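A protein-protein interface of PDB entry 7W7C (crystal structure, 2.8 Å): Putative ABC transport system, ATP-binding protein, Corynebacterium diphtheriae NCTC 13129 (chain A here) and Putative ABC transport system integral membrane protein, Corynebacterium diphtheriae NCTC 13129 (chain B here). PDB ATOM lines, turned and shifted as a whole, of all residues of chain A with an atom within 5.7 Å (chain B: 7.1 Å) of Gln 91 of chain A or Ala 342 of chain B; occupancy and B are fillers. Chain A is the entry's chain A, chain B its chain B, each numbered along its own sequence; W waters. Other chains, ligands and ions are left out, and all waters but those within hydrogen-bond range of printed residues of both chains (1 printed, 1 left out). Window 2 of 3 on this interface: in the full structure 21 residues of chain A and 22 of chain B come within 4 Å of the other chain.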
ATOM      1  N   VAL A  88       3.403  14.202   3.028  1.00  0.00           N
ATOM      2  CA  VAL A  88       3.225  15.149   4.128  1.00  0.00           C
ATOM      3  C   VAL A  88       2.479  16.344   3.539  1.00  0.00           C
ATOM      4  O   VAL A  88       3.077  17.326   3.076  1.00  0.00           O
ATOM      5  CB  VAL A  88       4.554  15.544   4.762  1.00  0.00           C
ATOM      6  CG1 VAL A  88       4.335  16.522   5.883  1.00  0.00           C
ATOM      7  CG2 VAL A  88       5.289  14.309   5.260  1.00  0.00           C
ATOM      8  N   PHE A  89       1.151  16.248   3.542  1.00  0.00           N
ATOM      9  CA  PHE A  89       0.309  17.280   2.962  1.00  0.00           C
ATOM     10  C   PHE A  89       0.421  18.577   3.754  1.00  0.00           C
ATOM     11  O   PHE A  89       0.811  18.591   4.930  1.00  0.00           O
ATOM     12  CB  PHE A  89      -1.153  16.846   2.949  1.00  0.00           C
ATOM     13  CG  PHE A  89      -1.419  15.584   2.182  1.00  0.00           C
ATOM     14  CD1 PHE A  89      -1.579  15.616   0.805  1.00  0.00           C
ATOM     15  CD2 PHE A  89      -1.552  14.377   2.847  1.00  0.00           C
ATOM     16  CE1 PHE A  89      -1.842  14.466   0.098  1.00  0.00           C
ATOM     17  CE2 PHE A  89      -1.822  13.218   2.151  1.00  0.00           C
ATOM     18  CZ  PHE A  89      -1.966  13.261   0.771  1.00  0.00           C
ATOM     19  N   GLN A  90       0.040  19.680   3.094  1.00  0.00           N
ATOM     20  CA  GLN A  90       0.033  20.971   3.773  1.00  0.00           C
ATOM     21  C   GLN A  90      -1.004  20.985   4.884  1.00  0.00           C
ATOM     22  O   GLN A  90      -0.703  21.349   6.025  1.00  0.00           O
ATOM     23  CB  GLN A  90      -0.218  22.099   2.780  1.00  0.00           C
ATOM     24  CG  GLN A  90       0.032  23.469   3.373  1.00  0.00           C
ATOM     25  CD  GLN A  90      -0.076  24.577   2.349  1.00  0.00           C
ATOM     26  OE1 GLN A  90      -0.378  24.341   1.179  1.00  0.00           O
ATOM     27  NE2 GLN A  90       0.169  25.804   2.792  1.00  0.00           N
ATOM     28  N   GLN A  91      -2.232  20.588   4.568  1.00  0.00           N
ATOM     29  CA  GLN A  91      -3.185  20.289   5.619  1.00  0.00           C
ATOM     30  C   GLN A  91      -2.872  18.910   6.192  1.00  0.00           C
ATOM     31  O   GLN A  91      -2.528  18.003   5.434  1.00  0.00           O
ATOM     32  CB  GLN A  91      -4.613  20.311   5.081  1.00  0.00           C
ATOM     33  CG  GLN A  91      -4.945  21.530   4.239  1.00  0.00           C
ATOM     34  CD  GLN A  91      -5.073  22.800   5.058  1.00  0.00           C
ATOM     35  OE1 GLN A  91      -4.406  23.801   4.787  1.00  0.00           O
ATOM     36  NE2 GLN A  91      -5.956  22.775   6.049  1.00  0.00           N
ATOM     37  N   PRO A  92      -2.941  18.737   7.513  1.00  0.00           N
ATOM     38  CA  PRO A  92      -2.697  17.404   8.099  1.00  0.00           C
ATOM     39  C   PRO A  92      -3.513  16.277   7.469  1.00  0.00           C
ATOM     40  O   PRO A  92      -3.029  15.140   7.417  1.00  0.00           O
ATOM     41  CB  PRO A  92      -3.047  17.625   9.576  1.00  0.00           C
ATOM     42  CG  PRO A  92      -2.650  19.044   9.816  1.00  0.00           C
ATOM     43  CD  PRO A  92      -2.992  19.788   8.547  1.00  0.00           C
ATOM     44  N   ASN A  93      -4.713  16.564   6.962  1.00  0.00           N
ATOM     45  CA  ASN A  93      -5.527  15.590   6.223  1.00  0.00           C
ATOM     46  C   ASN A  93      -5.660  14.275   6.989  1.00  0.00           C
ATOM     47  O   ASN A  93      -5.400  13.189   6.469  1.00  0.00           O
ATOM     48  CB  ASN A  93      -4.963  15.354   4.818  1.00  0.00           C
ATOM     49  CG  ASN A  93      -5.328  16.461   3.849  1.00  0.00           C
ATOM     50  OD1 ASN A  93      -5.919  17.467   4.236  1.00  0.00           O
ATOM     51  ND2 ASN A  93      -4.960  16.288   2.582  1.00  0.00           N
ATOM     52  N   GLN A 146       0.278  17.508  12.461  1.00  0.00           N
ATOM     53  CA  GLN A 146       1.311  17.421  11.437  1.00  0.00           C
ATOM     54  C   GLN A 146       2.291  16.287  11.728  1.00  0.00           C
ATOM     55  O   GLN A 146       2.740  15.588  10.808  1.00  0.00           O
ATOM     56  CB  GLN A 146       2.043  18.759  11.316  1.00  0.00           C
ATOM     57  CG  GLN A 146       1.420  19.726  10.319  1.00  0.00           C
ATOM     58  CD  GLN A 146       1.521  19.227   8.889  1.00  0.00           C
ATOM     59  OE1 GLN A 146       2.148  18.204   8.615  1.00  0.00           O
ATOM     60  NE2 GLN A 146       0.906  19.959   7.962  1.00  0.00           N
ATOM     61  N   ASN A 149       0.695  13.213  10.580  1.00  0.00           N
ATOM     62  CA  ASN A 149       0.790  13.195   9.123  1.00  0.00           C
ATOM     63  C   ASN A 149       2.139  12.641   8.660  1.00  0.00           C
ATOM     64  O   ASN A 149       2.207  11.801   7.747  1.00  0.00           O
ATOM     65  CB  ASN A 149       0.561  14.619   8.609  1.00  0.00           C
ATOM     66  CG  ASN A 149       0.461  14.705   7.106  1.00  0.00           C
ATOM     67  OD1 ASN A 149       0.195  13.719   6.422  1.00  0.00           O
ATOM     68  ND2 ASN A 149       0.667  15.907   6.580  1.00  0.00           N
ATOM     69  N   ARG A 152       2.378   8.895   9.388  1.00  0.00           N
ATOM     70  CA  ARG A 152       1.603   8.192   8.373  1.00  0.00           C
ATOM     71  C   ARG A 152       2.398   8.048   7.086  1.00  0.00           C
ATOM     72  O   ARG A 152       2.417   6.974   6.475  1.00  0.00           O
ATOM     73  CB  ARG A 152       0.291   8.929   8.104  1.00  0.00           C
ATOM     74  CG  ARG A 152      -0.465   8.404   6.893  1.00  0.00           C
ATOM     75  CD  ARG A 152      -1.800   9.112   6.716  1.00  0.00           C
ATOM     76  NE  ARG A 152      -1.633  10.539   6.458  1.00  0.00           N
ATOM     77  CZ  ARG A 152      -2.636  11.409   6.407  1.00  0.00           C
ATOM     78  NH1 ARG A 152      -3.880  10.992   6.604  1.00  0.00           N
ATOM     79  NH2 ARG A 152      -2.394  12.693   6.170  1.00  0.00           N
ATOM     80  N   ASP A 164       4.593  19.271   1.453  1.00  0.00           N
ATOM     81  CA  ASP A 164       4.049  20.473   0.828  1.00  0.00           C
ATOM     82  C   ASP A 164       3.804  21.504   1.923  1.00  0.00           C
ATOM     83  O   ASP A 164       2.772  21.470   2.594  1.00  0.00           O
ATOM     84  CB  ASP A 164       2.771  20.145   0.061  1.00  0.00           C
ATOM     85  CG  ASP A 164       2.205  21.349  -0.686  1.00  0.00           C
ATOM     86  OD1 ASP A 164       2.972  22.298  -0.961  1.00  0.00           O
ATOM     87  OD2 ASP A 164       0.990  21.352  -0.980  1.00  0.00           O
ATOM     88  N   SER A 168       2.975  25.646   7.329  1.00  0.00           N
ATOM     89  CA  SER A 168       2.337  26.901   6.946  1.00  0.00           C
ATOM     90  C   SER A 168       1.403  27.421   8.028  1.00  0.00           C
ATOM     91  O   SER A 168       1.186  28.633   8.127  1.00  0.00           O
ATOM     92  CB  SER A 168       1.574  26.737   5.634  1.00  0.00           C
ATOM     93  OG  SER A 168       0.490  25.837   5.792  1.00  0.00           O
ATOM     94  N   ARG B 251     -13.873  14.642   0.968  1.00  0.00           N
ATOM     95  CA  ARG B 251     -12.463  14.956   1.218  1.00  0.00           C
ATOM     96  C   ARG B 251     -11.695  13.789   1.838  1.00  0.00           C
ATOM     97  O   ARG B 251     -10.518  13.591   1.513  1.00  0.00           O
ATOM     98  CB  ARG B 251     -12.322  16.193   2.108  1.00  0.00           C
ATOM     99  CG  ARG B 251     -10.869  16.464   2.507  1.00  0.00           C
ATOM    100  CD  ARG B 251     -10.661  17.837   3.117  1.00  0.00           C
ATOM    101  NE  ARG B 251      -9.875  18.695   2.234  1.00  0.00           N
ATOM    102  CZ  ARG B 251      -8.548  18.793   2.263  1.00  0.00           C
ATOM    103  NH1 ARG B 251      -7.844  18.092   3.139  1.00  0.00           N
ATOM    104  NH2 ARG B 251      -7.927  19.600   1.414  1.00  0.00           N
ATOM    105  N   GLN B 337      -6.083  15.529  -6.108  1.00  0.00           N
ATOM    106  CA  GLN B 337      -5.439  16.822  -5.905  1.00  0.00           C
ATOM    107  C   GLN B 337      -6.250  17.724  -4.986  1.00  0.00           C
ATOM    108  O   GLN B 337      -5.735  18.754  -4.534  1.00  0.00           O
ATOM    109  CB  GLN B 337      -5.196  17.499  -7.251  1.00  0.00           C
ATOM    110  CG  GLN B 337      -4.636  16.544  -8.296  1.00  0.00           C
ATOM    111  CD  GLN B 337      -3.903  17.256  -9.411  1.00  0.00           C
ATOM    112  OE1 GLN B 337      -4.214  17.072 -10.589  1.00  0.00           O
ATOM    113  NE2 GLN B 337      -2.913  18.067  -9.047  1.00  0.00           N
ATOM    114  N   ILE B 338      -7.508  17.361  -4.714  1.00  0.00           N
ATOM    115  CA  ILE B 338      -8.288  18.022  -3.670  1.00  0.00           C
ATOM    116  C   ILE B 338      -7.527  17.994  -2.351  1.00  0.00           C
ATOM    117  O   ILE B 338      -7.547  18.960  -1.579  1.00  0.00           O
ATOM    118  CB  ILE B 338      -9.671  17.350  -3.543  1.00  0.00           C
ATOM    119  CG1 ILE B 338     -10.545  17.673  -4.760  1.00  0.00           C
ATOM    120  CG2 ILE B 338     -10.362  17.751  -2.246  1.00  0.00           C
ATOM    121  CD1 ILE B 338     -11.939  17.066  -4.699  1.00  0.00           C
ATOM    122  N   ALA B 339      -6.825  16.891  -2.086  1.00  0.00           N
ATOM    123  CA  ALA B 339      -6.056  16.774  -0.854  1.00  0.00           C
ATOM    124  C   ALA B 339      -4.929  17.797  -0.800  1.00  0.00           C
ATOM    125  O   ALA B 339      -4.511  18.203   0.293  1.00  0.00           O
ATOM    126  CB  ALA B 339      -5.506  15.352  -0.716  1.00  0.00           C
ATOM    127  N   LEU B 340      -4.445  18.244  -1.963  1.00  0.00           N
ATOM    128  CA  LEU B 340      -3.324  19.172  -2.003  1.00  0.00           C
ATOM    129  C   LEU B 340      -3.708  20.587  -1.594  1.00  0.00           C
ATOM    130  O   LEU B 340      -2.824  21.388  -1.281  1.00  0.00           O
ATOM    131  CB  LEU B 340      -2.701  19.182  -3.398  1.00  0.00           C
ATOM    132  CG  LEU B 340      -2.044  17.865  -3.801  1.00  0.00           C
ATOM    133  CD1 LEU B 340      -1.377  17.987  -5.161  1.00  0.00           C
ATOM    134  CD2 LEU B 340      -1.031  17.464  -2.742  1.00  0.00           C
ATOM    135  N   GLY B 341      -4.997  20.910  -1.580  1.00  0.00           N
ATOM    136  CA  GLY B 341      -5.427  22.260  -1.274  1.00  0.00           C
ATOM    137  C   GLY B 341      -5.377  22.600   0.202  1.00  0.00           C
ATOM    138  O   GLY B 341      -4.656  21.962   0.974  1.00  0.00           O
ATOM    139  N   ALA B 342      -6.148  23.610   0.600  1.00  0.00           N
ATOM    140  CA  ALA B 342      -6.184  24.051   1.987  1.00  0.00           C
ATOM    141  C   ALA B 342      -7.591  23.920   2.545  1.00  0.00           C
ATOM    142  O   ALA B 342      -8.563  23.936   1.793  1.00  0.00           O
ATOM    143  CB  ALA B 342      -5.693  25.487   2.103  1.00  0.00           C
HETATM  144  O   HOH W   1      -0.902  19.491   0.141  1.00  0.00           O
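ND2 of Asn 93 of chain A lies close to NH1 of Arg 251 of chain B (3.4 Å). The side-chain amide nitrogen of Asn 93 of chain A sits at hydrogen-bond distance from the backbone carbonyl oxygen of Ala 339 of chain B, at 3.0 Å.
N of Asp 164 of chain A sits at hydrogen-bond distance from O of Val 88 of chain A, 3.0 Å away. NE2 of Gln 146 of chain A lies within hydrogen-bond range of O of Phe 89 of chain A (3.3 Å). The backbone NH of Phe 89 of chain A sits close to the side-chain amide nitrogen of Asn 149 of chain A (3.1 Å). N of Gln 90 of chain A lies close to O of Asp 164 of chain A, 3.3 Å away. The backbone carbonyl oxygen (O) of Asn 93 of chain A lies within hydrogen-bond range of the guanidinium group (NH1) of Arg 152 of chain A (2.7 Å). The guanidinium group of Arg 251 of chain B sits at hydrogen-bond distance from the backbone carbonyl oxygen of Ile 338 of chain B (3.1 Å).
Among the printed residues, pairs that only touch across the chains: Phe 89 of chain A with Ala 339 of chain B (3.9 Å), Gln 91 of chain A with Gly 341 of chain B (3.3 Å), Gln 91 of chain A with Ala 342 of chain B (3.3 Å) and Asp 164 of chain A with Leu 340 of chain B (3.8 Å).
Gln 91 of chain A touches just these residues of chain B: Gly 341 and Ala 342. Of chain A, only Gln 91 (3.3 Å) comes within 4 Å of Ala 342 of chain B. Of the printed residues of chain A, Arg 251 of chain B touches Asn 93. Of the printed residues of chain A, Leu 340 of chain B touches Asp 164. Of the printed residues of chain B, Phe 89 of chain A touches Ala 339. The nearest residue of chain A that does not touch Ala 342 of chain B is Gln 90 of chain A (5.5 Å).
Printed residues of chain B that touch a printed residue of chain A: Arg 251, Ala 339, Leu 340, Gly 341 and Ala 342. Of the 11 printed residues of chain A, 4 touch a printed residue of chain B. Among the printed residues, no Asp or Glu carboxylate lies within 4 Å of a Lys or Arg side-chain nitrogen of the other chain.
Water W1 lies within hydrogen-bond range of OD2 of Asp 164 of chain A, O of Leu 340 of chain B and N of Gln 90 of chain A.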
